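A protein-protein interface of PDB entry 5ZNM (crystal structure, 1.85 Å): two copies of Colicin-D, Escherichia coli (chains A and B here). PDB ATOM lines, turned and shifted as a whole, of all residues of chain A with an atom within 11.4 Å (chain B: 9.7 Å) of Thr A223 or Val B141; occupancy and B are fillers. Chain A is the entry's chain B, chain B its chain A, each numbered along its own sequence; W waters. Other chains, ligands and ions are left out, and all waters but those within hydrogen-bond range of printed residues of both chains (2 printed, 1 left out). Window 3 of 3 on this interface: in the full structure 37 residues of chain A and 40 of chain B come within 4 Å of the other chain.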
ATOM      1  N   GLN A  32      20.048  28.469  24.271  1.00  0.00           N
ATOM      2  CA  GLN A  32      21.436  28.671  23.882  1.00  0.00           C
ATOM      3  C   GLN A  32      22.374  28.576  25.087  1.00  0.00           C
ATOM      4  O   GLN A  32      23.434  27.944  25.021  1.00  0.00           O
ATOM      5  CB  GLN A  32      21.549  30.034  23.189  1.00  0.00           C
ATOM      6  CG  GLN A  32      22.935  30.454  22.755  1.00  0.00           C
ATOM      7  CD  GLN A  32      23.502  29.587  21.652  1.00  0.00           C
ATOM      8  OE1 GLN A  32      22.762  29.002  20.856  1.00  0.00           O
ATOM      9  NE2 GLN A  32      24.826  29.502  21.595  1.00  0.00           N
ATOM     10  N   MET A  35      22.895  25.035  26.459  1.00  0.00           N
ATOM     11  CA  MET A  35      23.773  24.286  25.570  1.00  0.00           C
ATOM     12  C   MET A  35      25.226  24.647  25.814  1.00  0.00           C
ATOM     13  O   MET A  35      26.104  23.775  25.811  1.00  0.00           O
ATOM     14  CB  MET A  35      23.405  24.559  24.109  1.00  0.00           C
ATOM     15  CG  MET A  35      24.436  23.986  23.135  1.00  0.00           C
ATOM     16  SD  MET A  35      24.132  24.456  21.422  1.00  0.00           S
ATOM     17  CE  MET A  35      24.387  26.227  21.528  1.00  0.00           C
ATOM     18  N   VAL A 219      27.325  14.477  14.990  1.00  0.00           N
ATOM     19  CA  VAL A 219      27.130  15.894  15.318  1.00  0.00           C
ATOM     20  C   VAL A 219      26.264  16.545  14.245  1.00  0.00           C
ATOM     21  O   VAL A 219      26.573  16.422  13.046  1.00  0.00           O
ATOM     22  CB  VAL A 219      28.482  16.603  15.428  1.00  0.00           C
ATOM     23  CG1 VAL A 219      28.288  18.113  15.568  1.00  0.00           C
ATOM     24  CG2 VAL A 219      29.279  16.038  16.587  1.00  0.00           C
ATOM     25  N   PRO A 220      25.192  17.243  14.608  1.00  0.00           N
ATOM     26  CA  PRO A 220      24.432  17.994  13.597  1.00  0.00           C
ATOM     27  C   PRO A 220      25.250  19.169  13.076  1.00  0.00           C
ATOM     28  O   PRO A 220      25.850  19.911  13.854  1.00  0.00           O
ATOM     29  CB  PRO A 220      23.181  18.461  14.353  1.00  0.00           C
ATOM     30  CG  PRO A 220      23.536  18.340  15.822  1.00  0.00           C
ATOM     31  CD  PRO A 220      24.547  17.245  15.935  1.00  0.00           C
ATOM     32  N   THR A 221      25.288  19.317  11.752  1.00  0.00           N
ATOM     33  CA  THR A 221      25.912  20.494  11.155  1.00  0.00           C
ATOM     34  C   THR A 221      25.254  21.754  11.701  1.00  0.00           C
ATOM     35  O   THR A 221      24.025  21.839  11.774  1.00  0.00           O
ATOM     36  CB  THR A 221      25.783  20.462   9.632  1.00  0.00           C
ATOM     37  OG1 THR A 221      26.122  19.160   9.142  1.00  0.00           O
ATOM     38  CG2 THR A 221      26.707  21.485   8.996  1.00  0.00           C
ATOM     39  N   ASP A 222      26.071  22.735  12.085  1.00  0.00           N
ATOM     40  CA  ASP A 222      25.568  23.898  12.819  1.00  0.00           C
ATOM     41  C   ASP A 222      24.914  24.851  11.834  1.00  0.00           C
ATOM     42  O   ASP A 222      25.545  25.755  11.287  1.00  0.00           O
ATOM     43  CB  ASP A 222      26.677  24.586  13.601  1.00  0.00           C
ATOM     44  CG  ASP A 222      26.141  25.595  14.602  1.00  0.00           C
ATOM     45  OD1 ASP A 222      25.133  26.267  14.298  1.00  0.00           O
ATOM     46  OD2 ASP A 222      26.717  25.708  15.702  1.00  0.00           O
ATOM     47  N   THR A 223      23.620  24.650  11.619  1.00  0.00           N
ATOM     48  CA  THR A 223      22.848  25.436  10.674  1.00  0.00           C
ATOM     49  C   THR A 223      21.535  25.837  11.330  1.00  0.00           C
ATOM     50  O   THR A 223      21.210  25.416  12.448  1.00  0.00           O
ATOM     51  CB  THR A 223      22.591  24.656   9.376  1.00  0.00           C
ATOM     52  OG1 THR A 223      21.711  23.555   9.644  1.00  0.00           O
ATOM     53  CG2 THR A 223      23.901  24.120   8.818  1.00  0.00           C
ATOM     54  N   GLY A 224      20.779  26.661  10.623  1.00  0.00           N
ATOM     55  CA  GLY A 224      19.454  27.017  11.059  1.00  0.00           C
ATOM     56  C   GLY A 224      18.447  25.900  10.987  1.00  0.00           C
ATOM     57  O   GLY A 224      17.278  26.132  11.295  1.00  0.00           O
ATOM     58  N   ASN A 225      18.855  24.683  10.604  1.00  0.00           N
ATOM     59  CA  ASN A 225      17.896  23.588  10.559  1.00  0.00           C
ATOM     60  C   ASN A 225      17.785  22.839  11.878  1.00  0.00           C
ATOM     61  O   ASN A 225      16.969  21.920  11.985  1.00  0.00           O
ATOM     62  CB  ASN A 225      18.262  22.609   9.445  1.00  0.00           C
ATOM     63  CG  ASN A 225      18.267  23.265   8.096  1.00  0.00           C
ATOM     64  OD1 ASN A 225      17.627  24.292   7.903  1.00  0.00           O
ATOM     65  ND2 ASN A 225      19.008  22.693   7.161  1.00  0.00           N
ATOM     66  N   HIS A 226      18.572  23.203  12.883  1.00  0.00           N
ATOM     67  CA  HIS A 226      18.581  22.491  14.150  1.00  0.00           C
ATOM     68  C   HIS A 226      18.402  23.483  15.288  1.00  0.00           C
ATOM     69  O   HIS A 226      18.741  24.656  15.159  1.00  0.00           O
ATOM     70  CB  HIS A 226      19.888  21.727  14.358  1.00  0.00           C
ATOM     71  CG  HIS A 226      20.255  20.844  13.212  1.00  0.00           C
ATOM     72  ND1 HIS A 226      19.626  19.642  12.975  1.00  0.00           N
ATOM     73  CD2 HIS A 226      21.191  20.981  12.243  1.00  0.00           C
ATOM     74  CE1 HIS A 226      20.152  19.080  11.900  1.00  0.00           C
ATOM     75  NE2 HIS A 226      21.108  19.869  11.442  1.00  0.00           N
ATOM     76  N   GLN A 227      17.877  23.004  16.390  1.00  0.00           N
ATOM     77  CA  GLN A 227      17.769  23.817  17.591  1.00  0.00           C
ATOM     78  C   GLN A 227      18.917  23.489  18.539  1.00  0.00           C
ATOM     79  O   GLN A 227      19.589  22.464  18.370  1.00  0.00           O
ATOM     80  CB  GLN A 227      16.418  23.564  18.262  1.00  0.00           C
ATOM     81  CG  GLN A 227      15.243  23.806  17.323  1.00  0.00           C
ATOM     82  CD  GLN A 227      13.956  24.062  18.073  1.00  0.00           C
ATOM     83  OE1 GLN A 227      13.939  24.826  19.024  1.00  0.00           O
ATOM     84  NE2 GLN A 227      12.882  23.397  17.669  1.00  0.00           N
ATOM     85  N   PRO A 228      19.196  24.336  19.540  1.00  0.00           N
ATOM     86  CA  PRO A 228      20.376  24.086  20.393  1.00  0.00           C
ATOM     87  C   PRO A 228      20.240  22.776  21.160  1.00  0.00           C
ATOM     88  O   PRO A 228      19.196  22.492  21.743  1.00  0.00           O
ATOM     89  CB  PRO A 228      20.403  25.295  21.344  1.00  0.00           C
ATOM     90  CG  PRO A 228      19.566  26.364  20.647  1.00  0.00           C
ATOM     91  CD  PRO A 228      18.510  25.590  19.912  1.00  0.00           C
ATOM     92  N   VAL A 229      21.301  21.972  21.131  1.00  0.00           N
ATOM     93  CA  VAL A 229      21.429  20.754  21.936  1.00  0.00           C
ATOM     94  C   VAL A 229      22.883  20.598  22.335  1.00  0.00           C
ATOM     95  O   VAL A 229      23.785  21.104  21.650  1.00  0.00           O
ATOM     96  CB  VAL A 229      20.968  19.486  21.178  1.00  0.00           C
ATOM     97  CG1 VAL A 229      19.500  19.599  20.705  1.00  0.00           C
ATOM     98  CG2 VAL A 229      21.931  19.169  20.030  1.00  0.00           C
ATOM     99  N   VAL A 231      26.441  19.074  22.400  1.00  0.00           N
ATOM    100  CA  VAL A 231      27.200  18.357  21.384  1.00  0.00           C
ATOM    101  C   VAL A 231      28.294  17.575  22.101  1.00  0.00           C
ATOM    102  O   VAL A 231      29.235  18.165  22.646  1.00  0.00           O
ATOM    103  CB  VAL A 231      27.795  19.298  20.329  1.00  0.00           C
ATOM    104  CG1 VAL A 231      28.729  18.501  19.392  1.00  0.00           C
ATOM    105  CG2 VAL A 231      26.680  19.986  19.536  1.00  0.00           C
ATOM    106  N   LEU B  18      10.002  24.922  11.043  1.00  0.00           N
ATOM    107  CA  LEU B  18      10.941  24.130  10.241  1.00  0.00           C
ATOM    108  C   LEU B  18      10.236  22.972   9.566  1.00  0.00           C
ATOM    109  O   LEU B  18      10.468  22.689   8.380  1.00  0.00           O
ATOM    110  CB  LEU B  18      12.078  23.588  11.111  1.00  0.00           C
ATOM    111  CG  LEU B  18      13.200  24.541  11.489  1.00  0.00           C
ATOM    112  CD1 LEU B  18      14.038  23.956  12.618  1.00  0.00           C
ATOM    113  CD2 LEU B  18      14.063  24.822  10.274  1.00  0.00           C
ATOM    114  N   ALA B 132      21.965  14.545   2.685  1.00  0.00           N
ATOM    115  CA  ALA B 132      22.192  15.318   1.473  1.00  0.00           C
ATOM    116  C   ALA B 132      23.199  16.430   1.698  1.00  0.00           C
ATOM    117  O   ALA B 132      23.877  16.844   0.754  1.00  0.00           O
ATOM    118  CB  ALA B 132      20.880  15.916   0.971  1.00  0.00           C
ATOM    119  N   GLN B 133      23.297  16.932   2.930  1.00  0.00           N
ATOM    120  CA  GLN B 133      24.138  18.095   3.185  1.00  0.00           C
ATOM    121  C   GLN B 133      25.604  17.783   2.934  1.00  0.00           C
ATOM    122  O   GLN B 133      26.360  18.660   2.511  1.00  0.00           O
ATOM    123  CB  GLN B 133      23.913  18.590   4.616  1.00  0.00           C
ATOM    124  CG  GLN B 133      24.713  19.819   5.019  1.00  0.00           C
ATOM    125  CD  GLN B 133      24.517  21.011   4.088  1.00  0.00           C
ATOM    126  OE1 GLN B 133      23.391  21.372   3.723  1.00  0.00           O
ATOM    127  NE2 GLN B 133      25.624  21.645   3.719  1.00  0.00           N
ATOM    128  N   MET B 134      26.018  16.536   3.147  1.00  0.00           N
ATOM    129  CA  MET B 134      27.413  16.198   2.900  1.00  0.00           C
ATOM    130  C   MET B 134      27.749  16.112   1.416  1.00  0.00           C
ATOM    131  O   MET B 134      28.931  15.979   1.080  1.00  0.00           O
ATOM    132  CB  MET B 134      27.776  14.878   3.584  1.00  0.00           C
ATOM    133  CG  MET B 134      27.004  13.678   3.078  1.00  0.00           C
ATOM    134  SD  MET B 134      27.760  12.125   3.603  1.00  0.00           S
ATOM    135  CE  MET B 134      26.332  11.230   4.207  1.00  0.00           C
ATOM    136  N   LEU B 135      26.757  16.179   0.526  1.00  0.00           N
ATOM    137  CA  LEU B 135      27.003  16.167  -0.909  1.00  0.00           C
ATOM    138  C   LEU B 135      26.702  17.505  -1.558  1.00  0.00           C
ATOM    139  O   LEU B 135      26.705  17.603  -2.789  1.00  0.00           O
ATOM    140  CB  LEU B 135      26.170  15.081  -1.581  1.00  0.00           C
ATOM    141  CG  LEU B 135      26.102  13.776  -0.799  1.00  0.00           C
ATOM    142  CD1 LEU B 135      25.211  12.811  -1.544  1.00  0.00           C
ATOM    143  CD2 LEU B 135      27.498  13.196  -0.590  1.00  0.00           C
ATOM    144  N   ALA B 136      26.429  18.533  -0.763  1.00  0.00           N
ATOM    145  CA  ALA B 136      25.981  19.804  -1.301  1.00  0.00           C
ATOM    146  C   ALA B 136      27.141  20.538  -1.966  1.00  0.00           C
ATOM    147  O   ALA B 136      28.318  20.251  -1.724  1.00  0.00           O
ATOM    148  CB  ALA B 136      25.367  20.668  -0.193  1.00  0.00           C
ATOM    149  N   GLY B 137      26.782  21.522  -2.788  1.00  0.00           N
ATOM    150  CA  GLY B 137      27.738  22.273  -3.570  1.00  0.00           C
ATOM    151  C   GLY B 137      28.634  23.167  -2.728  1.00  0.00           C
ATOM    152  O   GLY B 137      28.527  23.264  -1.505  1.00  0.00           O
ATOM    153  N   GLN B 138      29.550  23.838  -3.426  1.00  0.00           N
ATOM    154  CA  GLN B 138      30.544  24.666  -2.759  1.00  0.00           C
ATOM    155  C   GLN B 138      29.853  25.802  -2.012  1.00  0.00           C
ATOM    156  O   GLN B 138      29.090  26.577  -2.603  1.00  0.00           O
ATOM    157  CB  GLN B 138      31.555  25.195  -3.781  1.00  0.00           C
ATOM    158  CG  GLN B 138      32.695  25.991  -3.174  1.00  0.00           C
ATOM    159  CD  GLN B 138      32.269  27.392  -2.821  1.00  0.00           C
ATOM    160  OE1 GLN B 138      31.418  27.967  -3.503  1.00  0.00           O
ATOM    161  NE2 GLN B 138      32.826  27.947  -1.744  1.00  0.00           N
ATOM    162  N   GLY B 139      30.107  25.878  -0.706  1.00  0.00           N
ATOM    163  CA  GLY B 139      29.538  26.914   0.133  1.00  0.00           C
ATOM    164  C   GLY B 139      28.069  26.750   0.437  1.00  0.00           C
ATOM    165  O   GLY B 139      27.459  27.681   0.976  1.00  0.00           O
ATOM    166  N   VAL B 140      27.489  25.587   0.139  1.00  0.00           N
ATOM    167  CA  VAL B 140      26.042  25.407   0.131  1.00  0.00           C
ATOM    168  C   VAL B 140      25.564  24.832   1.456  1.00  0.00           C
ATOM    169  O   VAL B 140      26.123  23.847   1.957  1.00  0.00           O
ATOM    170  CB  VAL B 140      25.598  24.512  -1.039  1.00  0.00           C
ATOM    171  CG1 VAL B 140      24.115  24.195  -0.923  1.00  0.00           C
ATOM    172  CG2 VAL B 140      25.880  25.208  -2.358  1.00  0.00           C
ATOM    173  N   VAL B 141      24.520  25.445   2.016  1.00  0.00           N
ATOM    174  CA  VAL B 141      23.714  24.861   3.087  1.00  0.00           C
ATOM    175  C   VAL B 141      22.316  24.648   2.527  1.00  0.00           C
ATOM    176  O   VAL B 141      21.681  25.603   2.068  1.00  0.00           O
ATOM    177  CB  VAL B 141      23.653  25.759   4.332  1.00  0.00           C
ATOM    178  CG1 VAL B 141      22.716  25.134   5.365  1.00  0.00           C
ATOM    179  CG2 VAL B 141      25.033  25.970   4.910  1.00  0.00           C
ATOM    180  N   ILE B 142      21.839  23.407   2.557  1.00  0.00           N
ATOM    181  CA  ILE B 142      20.529  23.086   1.997  1.00  0.00           C
ATOM    182  C   ILE B 142      19.448  23.552   2.968  1.00  0.00           C
ATOM    183  O   ILE B 142      19.421  23.120   4.122  1.00  0.00           O
ATOM    184  CB  ILE B 142      20.406  21.584   1.719  1.00  0.00           C
ATOM    185  CG1 ILE B 142      21.497  21.146   0.730  1.00  0.00           C
ATOM    186  CG2 ILE B 142      18.990  21.241   1.234  1.00  0.00           C
ATOM    187  CD1 ILE B 142      21.547  19.639   0.450  1.00  0.00           C
ATOM    188  N   GLU B 143      18.521  24.436   2.486  1.00  0.00           N
ATOM    189  CA  GLU B 143      17.512  24.992   3.390  1.00  0.00           C
ATOM    190  C   GLU B 143      16.112  24.455   3.089  1.00  0.00           C
ATOM    191  O   GLU B 143      15.730  24.315   1.921  1.00  0.00           O
ATOM    192  CB  GLU B 143      17.465  26.522   3.312  1.00  0.00           C
ATOM    193  CG  GLU B 143      18.787  27.224   3.130  1.00  0.00           C
ATOM    194  CD  GLU B 143      18.598  28.717   2.916  1.00  0.00           C
ATOM    195  OE1 GLU B 143      18.998  29.229   1.844  1.00  0.00           O
ATOM    196  OE2 GLU B 143      18.029  29.375   3.817  1.00  0.00           O
ATOM    197  N   PRO B 144      15.319  24.174   4.123  1.00  0.00           N
ATOM    198  CA  PRO B 144      13.942  23.715   3.891  1.00  0.00           C
ATOM    199  C   PRO B 144      13.121  24.794   3.206  1.00  0.00           C
ATOM    200  O   PRO B 144      13.256  25.985   3.499  1.00  0.00           O
ATOM    201  CB  PRO B 144      13.413  23.412   5.302  1.00  0.00           C
ATOM    202  CG  PRO B 144      14.359  24.060   6.241  1.00  0.00           C
ATOM    203  CD  PRO B 144      15.687  24.171   5.549  1.00  0.00           C
ATOM    204  N   GLY B 145      12.262  24.357   2.279  1.00  0.00           N
ATOM    205  CA  GLY B 145      11.489  25.238   1.432  1.00  0.00           C
ATOM    206  C   GLY B 145      11.935  25.206  -0.012  1.00  0.00           C
ATOM    207  O   GLY B 145      11.137  25.512  -0.903  1.00  0.00           O
ATOM    208  N   ALA B 146      13.186  24.838  -0.260  1.00  0.00           N
ATOM    209  CA  ALA B 146      13.646  24.681  -1.634  1.00  0.00           C
ATOM    210  C   ALA B 146      12.867  23.571  -2.334  1.00  0.00           C
ATOM    211  O   ALA B 146      12.504  22.558  -1.729  1.00  0.00           O
ATOM    212  CB  ALA B 146      15.146  24.369  -1.662  1.00  0.00           C
ATOM    213  N   SER B 148      14.269  22.365  -5.299  1.00  0.00           N
ATOM    214  CA  SER B 148      15.321  21.524  -5.847  1.00  0.00           C
ATOM    215  C   SER B 148      16.646  21.959  -5.242  1.00  0.00           C
ATOM    216  O   SER B 148      16.758  23.021  -4.629  1.00  0.00           O
ATOM    217  CB  SER B 148      15.356  21.574  -7.387  1.00  0.00           C
ATOM    218  OG  SER B 148      15.621  22.881  -7.861  1.00  0.00           O
ATOM    219  N   VAL B 149      17.650  21.103  -5.404  1.00  0.00           N
ATOM    220  CA  VAL B 149      18.990  21.336  -4.887  1.00  0.00           C
ATOM    221  C   VAL B 149      19.974  20.948  -5.979  1.00  0.00           C
ATOM    222  O   VAL B 149      19.844  19.878  -6.582  1.00  0.00           O
ATOM    223  CB  VAL B 149      19.261  20.520  -3.609  1.00  0.00           C
ATOM    224  CG1 VAL B 149      20.681  20.775  -3.105  1.00  0.00           C
ATOM    225  CG2 VAL B 149      18.218  20.820  -2.538  1.00  0.00           C
ATOM    226  N   ASN B 150      20.949  21.807  -6.243  1.00  0.00           N
ATOM    227  CA  ASN B 150      21.954  21.518  -7.255  1.00  0.00           C
ATOM    228  C   ASN B 150      23.072  20.690  -6.632  1.00  0.00           C
ATOM    229  O   ASN B 150      23.786  21.170  -5.747  1.00  0.00           O
ATOM    230  CB  ASN B 150      22.499  22.811  -7.858  1.00  0.00           C
ATOM    231  CG  ASN B 150      21.589  23.389  -8.937  1.00  0.00           C
ATOM    232  OD1 ASN B 150      20.470  22.923  -9.155  1.00  0.00           O
ATOM    233  ND2 ASN B 150      22.071  24.419  -9.614  1.00  0.00           N
ATOM    234  N   LEU B 151      23.225  19.452  -7.095  1.00  0.00           N
ATOM    235  CA  LEU B 151      24.309  18.665  -6.551  1.00  0.00           C
ATOM    236  C   LEU B 151      25.425  18.535  -7.567  1.00  0.00           C
ATOM    237  O   LEU B 151      25.174  18.331  -8.761  1.00  0.00           O
ATOM    238  CB  LEU B 151      23.855  17.260  -6.136  1.00  0.00           C
ATOM    239  CG  LEU B 151      22.833  17.191  -5.007  1.00  0.00           C
ATOM    240  CD1 LEU B 151      22.624  15.739  -4.573  1.00  0.00           C
ATOM    241  CD2 LEU B 151      23.277  18.047  -3.840  1.00  0.00           C
ATOM    242  N   TRP B 265      13.011  15.526   3.394  1.00  0.00           N
ATOM    243  CA  TRP B 265      13.394  15.940   4.742  1.00  0.00           C
ATOM    244  C   TRP B 265      12.822  14.983   5.784  1.00  0.00           C
ATOM    245  O   TRP B 265      11.687  14.524   5.639  1.00  0.00           O
ATOM    246  CB  TRP B 265      12.882  17.349   5.042  1.00  0.00           C
ATOM    247  CG  TRP B 265      13.481  18.400   4.202  1.00  0.00           C
ATOM    248  CD1 TRP B 265      13.017  18.850   2.997  1.00  0.00           C
ATOM    249  CD2 TRP B 265      14.660  19.152   4.490  1.00  0.00           C
ATOM    250  NE1 TRP B 265      13.836  19.837   2.519  1.00  0.00           N
ATOM    251  CE2 TRP B 265      14.853  20.046   3.417  1.00  0.00           C
ATOM    252  CE3 TRP B 265      15.571  19.160   5.558  1.00  0.00           C
ATOM    253  CZ2 TRP B 265      15.918  20.936   3.371  1.00  0.00           C
ATOM    254  CZ3 TRP B 265      16.632  20.050   5.516  1.00  0.00           C
ATOM    255  CH2 TRP B 265      16.797  20.927   4.422  1.00  0.00           C
ATOM    256  N   ASP B 268      15.544  15.668  12.580  1.00  0.00           N
ATOM    257  CA  ASP B 268      16.914  15.401  12.986  1.00  0.00           C
ATOM    258  C   ASP B 268      16.937  14.497  14.220  1.00  0.00           C
ATOM    259  O   ASP B 268      15.900  14.050  14.727  1.00  0.00           O
ATOM    260  CB  ASP B 268      17.681  16.707  13.205  1.00  0.00           C
ATOM    261  CG  ASP B 268      17.090  17.584  14.315  1.00  0.00           C
ATOM    262  OD1 ASP B 268      16.206  17.132  15.065  1.00  0.00           O
ATOM    263  OD2 ASP B 268      17.530  18.746  14.422  1.00  0.00           O
ATOM    264  N   THR B 272      13.696  17.878  16.938  1.00  0.00           N
ATOM    265  CA  THR B 272      13.163  19.235  16.974  1.00  0.00           C
ATOM    266  C   THR B 272      13.571  20.064  15.769  1.00  0.00           C
ATOM    267  O   THR B 272      13.108  21.201  15.628  1.00  0.00           O
ATOM    268  CB  THR B 272      13.623  19.943  18.260  1.00  0.00           C
ATOM    269  OG1 THR B 272      15.056  19.890  18.345  1.00  0.00           O
ATOM    270  CG2 THR B 272      13.009  19.253  19.469  1.00  0.00           C
ATOM    271  N   GLY B 273      14.437  19.533  14.913  1.00  0.00           N
ATOM    272  CA  GLY B 273      14.840  20.184  13.684  1.00  0.00           C
ATOM    273  C   GLY B 273      14.749  19.200  12.529  1.00  0.00           C
ATOM    274  O   GLY B 273      14.091  18.163  12.662  1.00  0.00           O
ATOM    275  N   VAL B 274      15.389  19.495  11.395  1.00  0.00           N
ATOM    276  CA  VAL B 274      15.221  18.690  10.187  1.00  0.00           C
ATOM    277  C   VAL B 274      16.565  18.446   9.514  1.00  0.00           C
ATOM    278  O   VAL B 274      17.535  19.184   9.711  1.00  0.00           O
ATOM    279  CB  VAL B 274      14.243  19.338   9.164  1.00  0.00           C
ATOM    280  CG1 VAL B 274      12.851  19.494   9.766  1.00  0.00           C
ATOM    281  CG2 VAL B 274      14.760  20.679   8.693  1.00  0.00           C
ATOM    282  N   GLU B 275      16.609  17.388   8.696  1.00  0.00           N
ATOM    283  CA  GLU B 275      17.801  17.073   7.920  1.00  0.00           C
ATOM    284  C   GLU B 275      17.393  16.564   6.550  1.00  0.00           C
ATOM    285  O   GLU B 275      16.414  15.823   6.418  1.00  0.00           O
ATOM    286  CB  GLU B 275      18.691  16.022   8.613  1.00  0.00           C
ATOM    287  CG  GLU B 275      17.997  14.744   8.973  1.00  0.00           C
ATOM    288  CD  GLU B 275      18.959  13.687   9.518  1.00  0.00           C
ATOM    289  OE1 GLU B 275      19.888  14.036  10.289  1.00  0.00           O
ATOM    290  OE2 GLU B 275      18.773  12.507   9.179  1.00  0.00           O
ATOM    291  N   ALA B 276      18.139  16.983   5.533  1.00  0.00           N
ATOM    292  CA  ALA B 276      17.855  16.590   4.160  1.00  0.00           C
ATOM    293  C   ALA B 276      18.525  15.253   3.853  1.00  0.00           C
ATOM    294  O   ALA B 276      19.669  15.009   4.251  1.00  0.00           O
ATOM    295  CB  ALA B 276      18.348  17.657   3.180  1.00  0.00           C
HETATM  296  O   HOH W   1      21.121  21.311   5.196  1.00  0.00           O
HETATM  297  O   HOH W   2      17.160  20.229  16.589  1.00  0.00           O
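No position is printed for both chains.
CG2 of Thr A223 touches CG1 of Val B141 (3.8 Å). Leu B18 touches Gly A224 (CD2 to O, 3.6 Å). Leu B18 touches Asn A225 (CD1 to O, 3.6 Å). Pro B144 touches Asn A225 (CD to OD1, 3.1 Å). Trp B265 touches Asn A225 (CZ3 to ND2, 3.9 Å). Gly B273 touches Asn A225 (CA to O, 3.2 Å). O of Val B274 touches CE1 of His A226, 3.4 Å away.
Of the 14 printed residues of chain A, 5 touch a printed residue of chain B. Hydrophobic or aromatic side chains of chain A that line the printed part of chain B: His A226. Among the printed residues, 11 pairs touch across the chains.
Thr A223 touches one residue of chain B. No residue of chain B comes within 4 Å of Thr A221. No residue of chain B comes within 4 Å of Asp A222. Asn A225 touches just these residues of chain B: Leu B18, Ile B142, Pro B144, Trp B265, Gly B273 and Val B274. Of chain B, only Asp B268 (2.7 Å) and Val B274 (3.4 Å) come within 4 Å of His A226. Gly B139 touches none of the printed residues of chain A. Printed residues of chain A within 4 Å of Ile B142: Asn A225 (3.1 Å). Glu B143 touches none of the printed residues of chain A. Of the printed residues of chain B, Gln A227 touches Thr B272. Of the printed residues of chain A, Pro B144 touches Asn A225. Of the printed residues of chain A, Leu B18 touches Gly A224 (3.6 Å) and Asn A225 (3.6 Å). Printed residues of chain A within 4 Å of Gly B273: Asn A225 (3.2 Å). Ala B276 touches none of the printed residues of chain A. Val A231 touches none of the printed residues of chain B. The nearest printed residue of chain A that does not touch Asp B268 is Asn A225 (4.04 Å).
O of Thr B272 lies within hydrogen-bond range of NE2 of Gln A227, at 3.0 Å. ND2 of Asn A225 lies within hydrogen-bond range of O of Ile B142 (3.1 Å). OD2 of Asp B268 is in hydrogen-bond range of ND1 of His A226, at 2.7 Å. N of Val B274 lies within hydrogen-bond range of O of Asn A225, 3.0 Å away.
Water W2 lies within hydrogen-bond range of OD2 of Asp B268 (2.7 Å), OG1 of Thr B272 (2.8 Å), N of Gln A227 (2.9 Å) and N of Gly B273 (3.3 Å). Water W1 lies within hydrogen-bond range of O of Ile B142, OE1 of Gln B133 and ND2 of Asn A225.
N of Ile B142 sits at hydrogen-bond distance from OE1 of Gln B133 (2.8 Å). The side-chain carboxylate (OD1) of Asp B268 sits at hydrogen-bond distance from the backbone NH (N) of Thr B272, 3.2 Å away. The backbone NH of Asp B268 sits at hydrogen-bond distance from the backbone carbonyl oxygen of Gly B273, 2.9 Å away. The side-chain hydroxyl (OG1) of Thr A223 sits close to the backbone NH (N) of Asn A225 (3.2 Å).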
